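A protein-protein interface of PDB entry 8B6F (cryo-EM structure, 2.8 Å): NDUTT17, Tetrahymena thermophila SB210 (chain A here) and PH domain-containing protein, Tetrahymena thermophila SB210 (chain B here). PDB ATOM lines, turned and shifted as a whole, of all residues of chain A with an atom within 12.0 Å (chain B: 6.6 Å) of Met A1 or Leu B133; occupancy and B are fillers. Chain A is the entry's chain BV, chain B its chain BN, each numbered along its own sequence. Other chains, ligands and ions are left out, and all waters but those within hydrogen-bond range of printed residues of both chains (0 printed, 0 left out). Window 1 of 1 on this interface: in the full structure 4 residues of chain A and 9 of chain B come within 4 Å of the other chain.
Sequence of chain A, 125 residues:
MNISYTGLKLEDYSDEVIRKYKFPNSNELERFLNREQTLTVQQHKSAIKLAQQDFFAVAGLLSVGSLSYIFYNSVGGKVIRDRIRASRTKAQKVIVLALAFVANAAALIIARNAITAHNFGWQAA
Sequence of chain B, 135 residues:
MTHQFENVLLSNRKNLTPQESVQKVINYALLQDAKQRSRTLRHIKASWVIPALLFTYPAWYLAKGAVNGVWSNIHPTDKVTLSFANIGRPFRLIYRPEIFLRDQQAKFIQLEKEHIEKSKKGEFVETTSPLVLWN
Of the printed residues of chain B, Asn A2 touches Ile B109 and Glu B112.
Printed residues of chain A within 4 Å of Arg B102: Met A1 (3.1 Å).
No residue of chain A comes within 4 Å of Gln B105.
No residue of chain A comes within 4 Å of Phe B108.
Of chain A, only Asn A2 (3.6 Å) comes within 4 Å of Ile B109.
No residue of chain A comes within 4 Å of Leu B131.
No residue of chain A comes within 4 Å of Val B132.
Of the printed residues of chain A, Leu B133 touches Met A1 and Ile A3.
Trp B134 touches just these residues of chain A: Met A1 (3.5 Å) and Ile A3 (3.5 Å).
The nearest residue of chain A that does not touch Leu B133 is Asn A2 (5.3 Å).
SD of Met A1 sits close to O of Leu B133 (3.8 Å).
The side-chain carboxylate (OE1) of Glu B112 lies close to the side-chain amide oxygen (OD1) of Asn A2, 3.1 Å away.
SD of Met A1 sits close to N of Ile A3.
OE1 of Gln B105 lies close to O of Asn B135, at 2.6 Å.
Hydrophobic or aromatic side chains of chain B that line the printed part of chain A: Ile B109 and Trp B134.
Among the printed residues, no Asp or Glu carboxylate lies within 4 Å of a Lys or Arg side-chain nitrogen of the other chain.
Among the printed residues, pairs that only touch across the chains: Met A1 with Arg B102 (3.1 Å), Ile A3 with Leu B133 (3.2 Å), Ile A3 with Trp B134 (3.5 Å), Met A1 with Trp B134 (3.5 Å), Asn A2 with Ile B109 (3.6 Å) and Met A1 with Asn B135 (3.8 Å).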
ATOM      1  N   MET A   1      27.824  15.665 -17.374  1.00  0.00           N
ATOM      2  CA  MET A   1      28.735  15.184 -16.297  1.00  0.00           C
ATOM      3  C   MET A   1      29.055  16.313 -15.326  1.00  0.00           C
ATOM      4  O   MET A   1      29.602  17.344 -15.714  1.00  0.00           O
ATOM      5  CB  MET A   1      30.026  14.626 -16.900  1.00  0.00           C
ATOM      6  CG  MET A   1      31.034  14.132 -15.874  1.00  0.00           C
ATOM      7  SD  MET A   1      30.337  12.970 -14.683  1.00  0.00           S
ATOM      8  CE  MET A   1      29.664  11.721 -15.774  1.00  0.00           C
ATOM      9  N   ASN A   2      28.710  16.109 -14.057  1.00  0.00           N
ATOM     10  CA  ASN A   2      28.885  17.120 -13.026  1.00  0.00           C
ATOM     11  C   ASN A   2      30.185  16.965 -12.248  1.00  0.00           C
ATOM     12  O   ASN A   2      30.441  17.755 -11.336  1.00  0.00           O
ATOM     13  CB  ASN A   2      27.700  17.082 -12.058  1.00  0.00           C
ATOM     14  CG  ASN A   2      26.367  17.097 -12.775  1.00  0.00           C
ATOM     15  OD1 ASN A   2      25.786  16.048 -13.049  1.00  0.00           O
ATOM     16  ND2 ASN A   2      25.877  18.289 -13.091  1.00  0.00           N
ATOM     17  N   ILE A   3      31.007  15.978 -12.582  1.00  0.00           N
ATOM     18  CA  ILE A   3      32.269  15.737 -11.885  1.00  0.00           C
ATOM     19  C   ILE A   3      33.346  16.440 -12.703  1.00  0.00           C
ATOM     20  O   ILE A   3      33.943  15.867 -13.615  1.00  0.00           O
ATOM     21  CB  ILE A   3      32.548  14.245 -11.714  1.00  0.00           C
ATOM     22  CG1 ILE A   3      31.419  13.591 -10.911  1.00  0.00           C
ATOM     23  CG2 ILE A   3      33.890  14.033 -11.026  1.00  0.00           C
ATOM     24  CD1 ILE A   3      31.541  12.090 -10.777  1.00  0.00           C
ATOM     25  N   SER A   4      33.601  17.702 -12.368  1.00  0.00           N
ATOM     26  CA  SER A   4      34.602  18.491 -13.070  1.00  0.00           C
ATOM     27  C   SER A   4      35.061  19.616 -12.157  1.00  0.00           C
ATOM     28  O   SER A   4      34.418  19.926 -11.151  1.00  0.00           O
ATOM     29  CB  SER A   4      34.057  19.050 -14.388  1.00  0.00           C
ATOM     30  OG  SER A   4      32.955  19.911 -14.161  1.00  0.00           O
ATOM     31  N   TYR A   5      36.189  20.225 -12.525  1.00  0.00           N
ATOM     32  CA  TYR A   5      36.737  21.335 -11.756  1.00  0.00           C
ATOM     33  C   TYR A   5      35.914  22.609 -11.883  1.00  0.00           C
ATOM     34  O   TYR A   5      36.143  23.549 -11.114  1.00  0.00           O
ATOM     35  CB  TYR A   5      38.172  21.619 -12.197  1.00  0.00           C
ATOM     36  CG  TYR A   5      39.159  20.536 -11.835  1.00  0.00           C
ATOM     37  CD1 TYR A   5      39.738  20.490 -10.575  1.00  0.00           C
ATOM     38  CD2 TYR A   5      39.521  19.567 -12.759  1.00  0.00           C
ATOM     39  CE1 TYR A   5      40.646  19.505 -10.242  1.00  0.00           C
ATOM     40  CE2 TYR A   5      40.428  18.576 -12.435  1.00  0.00           C
ATOM     41  CZ  TYR A   5      40.988  18.553 -11.175  1.00  0.00           C
ATOM     42  OH  TYR A   5      41.890  17.571 -10.847  1.00  0.00           O
ATOM     43  N   THR A   6      34.978  22.671 -12.825  1.00  0.00           N
ATOM     44  CA  THR A   6      34.210  23.892 -13.034  1.00  0.00           C
ATOM     45  C   THR A   6      33.401  24.237 -11.789  1.00  0.00           C
ATOM     46  O   THR A   6      32.729  23.379 -11.210  1.00  0.00           O
ATOM     47  CB  THR A   6      33.279  23.725 -14.235  1.00  0.00           C
ATOM     48  OG1 THR A   6      34.046  23.386 -15.397  1.00  0.00           O
ATOM     49  CG2 THR A   6      32.503  25.009 -14.504  1.00  0.00           C
ATOM     50  N   GLY A   7      33.465  25.504 -11.383  1.00  0.00           N
ATOM     51  CA  GLY A   7      32.694  25.988 -10.260  1.00  0.00           C
ATOM     52  C   GLY A   7      33.321  25.776  -8.901  1.00  0.00           C
ATOM     53  O   GLY A   7      32.735  26.206  -7.898  1.00  0.00           O
ATOM     54  N   LEU A   8      34.486  25.138  -8.824  1.00  0.00           N
ATOM     55  CA  LEU A   8      35.122  24.851  -7.546  1.00  0.00           C
ATOM     56  C   LEU A   8      36.058  25.988  -7.160  1.00  0.00           C
ATOM     57  O   LEU A   8      36.845  26.461  -7.985  1.00  0.00           O
ATOM     58  CB  LEU A   8      35.899  23.536  -7.619  1.00  0.00           C
ATOM     59  CG  LEU A   8      35.095  22.293  -8.012  1.00  0.00           C
ATOM     60  CD1 LEU A   8      35.973  21.055  -7.951  1.00  0.00           C
ATOM     61  CD2 LEU A   8      33.867  22.123  -7.146  1.00  0.00           C
ATOM     62  N   ARG B 102      24.081   7.298 -20.047  1.00  0.00           N
ATOM     63  CA  ARG B 102      23.798   8.727 -19.947  1.00  0.00           C
ATOM     64  C   ARG B 102      22.351   9.032 -20.318  1.00  0.00           C
ATOM     65  O   ARG B 102      21.701   9.855 -19.666  1.00  0.00           O
ATOM     66  CB  ARG B 102      24.763   9.522 -20.821  1.00  0.00           C
ATOM     67  CG  ARG B 102      24.644  11.026 -20.628  1.00  0.00           C
ATOM     68  CD  ARG B 102      25.974  11.735 -20.815  1.00  0.00           C
ATOM     69  NE  ARG B 102      26.966  11.305 -19.837  1.00  0.00           N
ATOM     70  CZ  ARG B 102      28.182  11.820 -19.725  1.00  0.00           C
ATOM     71  NH1 ARG B 102      28.590  12.807 -20.507  1.00  0.00           N
ATOM     72  NH2 ARG B 102      29.013  11.331 -18.810  1.00  0.00           N
ATOM     73  N   GLN B 105      20.272   8.156 -17.480  1.00  0.00           N
ATOM     74  CA  GLN B 105      20.452   9.064 -16.356  1.00  0.00           C
ATOM     75  C   GLN B 105      20.085  10.500 -16.690  1.00  0.00           C
ATOM     76  O   GLN B 105      20.319  11.390 -15.867  1.00  0.00           O
ATOM     77  CB  GLN B 105      21.901   9.017 -15.872  1.00  0.00           C
ATOM     78  CG  GLN B 105      22.318   7.678 -15.341  1.00  0.00           C
ATOM     79  CD  GLN B 105      23.805   7.583 -15.094  1.00  0.00           C
ATOM     80  OE1 GLN B 105      24.524   8.576 -15.178  1.00  0.00           O
ATOM     81  NE2 GLN B 105      24.275   6.381 -14.783  1.00  0.00           N
ATOM     82  N   PHE B 108      18.425  12.356 -13.941  1.00  0.00           N
ATOM     83  CA  PHE B 108      19.279  12.361 -12.760  1.00  0.00           C
ATOM     84  C   PHE B 108      20.427  13.351 -12.900  1.00  0.00           C
ATOM     85  O   PHE B 108      20.902  13.895 -11.897  1.00  0.00           O
ATOM     86  CB  PHE B 108      19.818  10.955 -12.496  1.00  0.00           C
ATOM     87  CG  PHE B 108      18.747   9.929 -12.251  1.00  0.00           C
ATOM     88  CD1 PHE B 108      17.540  10.284 -11.667  1.00  0.00           C
ATOM     89  CD2 PHE B 108      18.948   8.606 -12.605  1.00  0.00           C
ATOM     90  CE1 PHE B 108      16.557   9.338 -11.443  1.00  0.00           C
ATOM     91  CE2 PHE B 108      17.970   7.657 -12.384  1.00  0.00           C
ATOM     92  CZ  PHE B 108      16.772   8.024 -11.802  1.00  0.00           C
ATOM     93  N   ILE B 109      20.884  13.600 -14.128  1.00  0.00           N
ATOM     94  CA  ILE B 109      21.954  14.571 -14.336  1.00  0.00           C
ATOM     95  C   ILE B 109      21.496  15.960 -13.914  1.00  0.00           C
ATOM     96  O   ILE B 109      22.209  16.677 -13.204  1.00  0.00           O
ATOM     97  CB  ILE B 109      22.423  14.553 -15.804  1.00  0.00           C
ATOM     98  CG1 ILE B 109      23.006  13.186 -16.181  1.00  0.00           C
ATOM     99  CG2 ILE B 109      23.452  15.654 -16.056  1.00  0.00           C
ATOM    100  CD1 ILE B 109      24.237  12.780 -15.400  1.00  0.00           C
ATOM    101  N   GLU B 112      21.132  16.164 -10.142  1.00  0.00           N
ATOM    102  CA  GLU B 112      22.431  16.327  -9.500  1.00  0.00           C
ATOM    103  C   GLU B 112      22.956  17.744  -9.680  1.00  0.00           C
ATOM    104  O   GLU B 112      23.548  18.316  -8.759  1.00  0.00           O
ATOM    105  CB  GLU B 112      23.420  15.311 -10.070  1.00  0.00           C
ATOM    106  CG  GLU B 112      24.790  15.342  -9.412  1.00  0.00           C
ATOM    107  CD  GLU B 112      25.757  14.362 -10.047  1.00  0.00           C
ATOM    108  OE1 GLU B 112      25.374  13.709 -11.040  1.00  0.00           O
ATOM    109  OE2 GLU B 112      26.900  14.247  -9.555  1.00  0.00           O
ATOM    110  N   PRO B 130      21.857  11.001  -2.805  1.00  0.00           N
ATOM    111  CA  PRO B 130      22.499   9.787  -3.335  1.00  0.00           C
ATOM    112  C   PRO B 130      22.938   9.909  -4.784  1.00  0.00           C
ATOM    113  O   PRO B 130      23.831   9.166  -5.207  1.00  0.00           O
ATOM    114  CB  PRO B 130      21.415   8.711  -3.168  1.00  0.00           C
ATOM    115  CG  PRO B 130      20.454   9.266  -2.182  1.00  0.00           C
ATOM    116  CD  PRO B 130      20.464  10.739  -2.404  1.00  0.00           C
ATOM    117  N   LEU B 131      22.345  10.818  -5.557  1.00  0.00           N
ATOM    118  CA  LEU B 131      22.619  10.923  -6.990  1.00  0.00           C
ATOM    119  C   LEU B 131      23.979  11.581  -7.198  1.00  0.00           C
ATOM    120  O   LEU B 131      24.104  12.789  -7.415  1.00  0.00           O
ATOM    121  CB  LEU B 131      21.510  11.697  -7.691  1.00  0.00           C
ATOM    122  CG  LEU B 131      20.142  11.014  -7.736  1.00  0.00           C
ATOM    123  CD1 LEU B 131      19.102  11.952  -8.319  1.00  0.00           C
ATOM    124  CD2 LEU B 131      20.201   9.725  -8.540  1.00  0.00           C
ATOM    125  N   VAL B 132      25.018  10.760  -7.129  1.00  0.00           N
ATOM    126  CA  VAL B 132      26.383  11.168  -7.456  1.00  0.00           C
ATOM    127  C   VAL B 132      26.854  10.219  -8.551  1.00  0.00           C
ATOM    128  O   VAL B 132      27.359   9.127  -8.283  1.00  0.00           O
ATOM    129  CB  VAL B 132      27.312  11.143  -6.241  1.00  0.00           C
ATOM    130  CG1 VAL B 132      28.702  11.623  -6.621  1.00  0.00           C
ATOM    131  CG2 VAL B 132      26.740  12.006  -5.132  1.00  0.00           C
ATOM    132  N   LEU B 133      26.692  10.641  -9.800  1.00  0.00           N
ATOM    133  CA  LEU B 133      26.933   9.793 -10.957  1.00  0.00           C
ATOM    134  C   LEU B 133      28.246  10.169 -11.627  1.00  0.00           C
ATOM    135  O   LEU B 133      28.593  11.350 -11.721  1.00  0.00           O
ATOM    136  CB  LEU B 133      25.785   9.923 -11.959  1.00  0.00           C
ATOM    137  CG  LEU B 133      24.382   9.724 -11.380  1.00  0.00           C
ATOM    138  CD1 LEU B 133      23.327  10.112 -12.397  1.00  0.00           C
ATOM    139  CD2 LEU B 133      24.184   8.288 -10.928  1.00  0.00           C
ATOM    140  N   TRP B 134      28.977   9.152 -12.092  1.00  0.00           N
ATOM    141  CA  TRP B 134      30.237   9.354 -12.793  1.00  0.00           C
ATOM    142  C   TRP B 134      30.258   8.682 -14.161  1.00  0.00           C
ATOM    143  O   TRP B 134      31.309   8.664 -14.810  1.00  0.00           O
ATOM    144  CB  TRP B 134      31.407   8.834 -11.950  1.00  0.00           C
ATOM    145  CG  TRP B 134      31.275   7.392 -11.588  1.00  0.00           C
ATOM    146  CD1 TRP B 134      30.674   6.881 -10.479  1.00  0.00           C
ATOM    147  CD2 TRP B 134      31.755   6.271 -12.340  1.00  0.00           C
ATOM    148  NE1 TRP B 134      30.747   5.509 -10.492  1.00  0.00           N
ATOM    149  CE2 TRP B 134      31.405   5.110 -11.625  1.00  0.00           C
ATOM    150  CE3 TRP B 134      32.443   6.137 -13.549  1.00  0.00           C
ATOM    151  CZ2 TRP B 134      31.722   3.832 -12.076  1.00  0.00           C
ATOM    152  CZ3 TRP B 134      32.756   4.867 -13.998  1.00  0.00           C
ATOM    153  CH2 TRP B 134      32.395   3.729 -13.263  1.00  0.00           C
ATOM    154  N   ASN B 135      29.136   8.135 -14.617  1.00  0.00           N
ATOM    155  CA  ASN B 135      29.080   7.471 -15.914  1.00  0.00           C
ATOM    156  C   ASN B 135      27.652   7.414 -16.444  1.00  0.00           C
ATOM    157  O   ASN B 135      26.697   7.294 -15.679  1.00  0.00           O
ATOM    158  CB  ASN B 135      29.654   6.059 -15.817  1.00  0.00           C
ATOM    159  CG  ASN B 135      28.961   5.223 -14.761  1.00  0.00           C
ATOM    160  OD1 ASN B 135      27.918   5.605 -14.233  1.00  0.00           O
ATOM    161  ND2 ASN B 135      29.538   4.070 -14.449  1.00  0.00           N
ATOM    162  OXT ASN B 135      27.419   7.474 -17.651  1.00  0.00           O
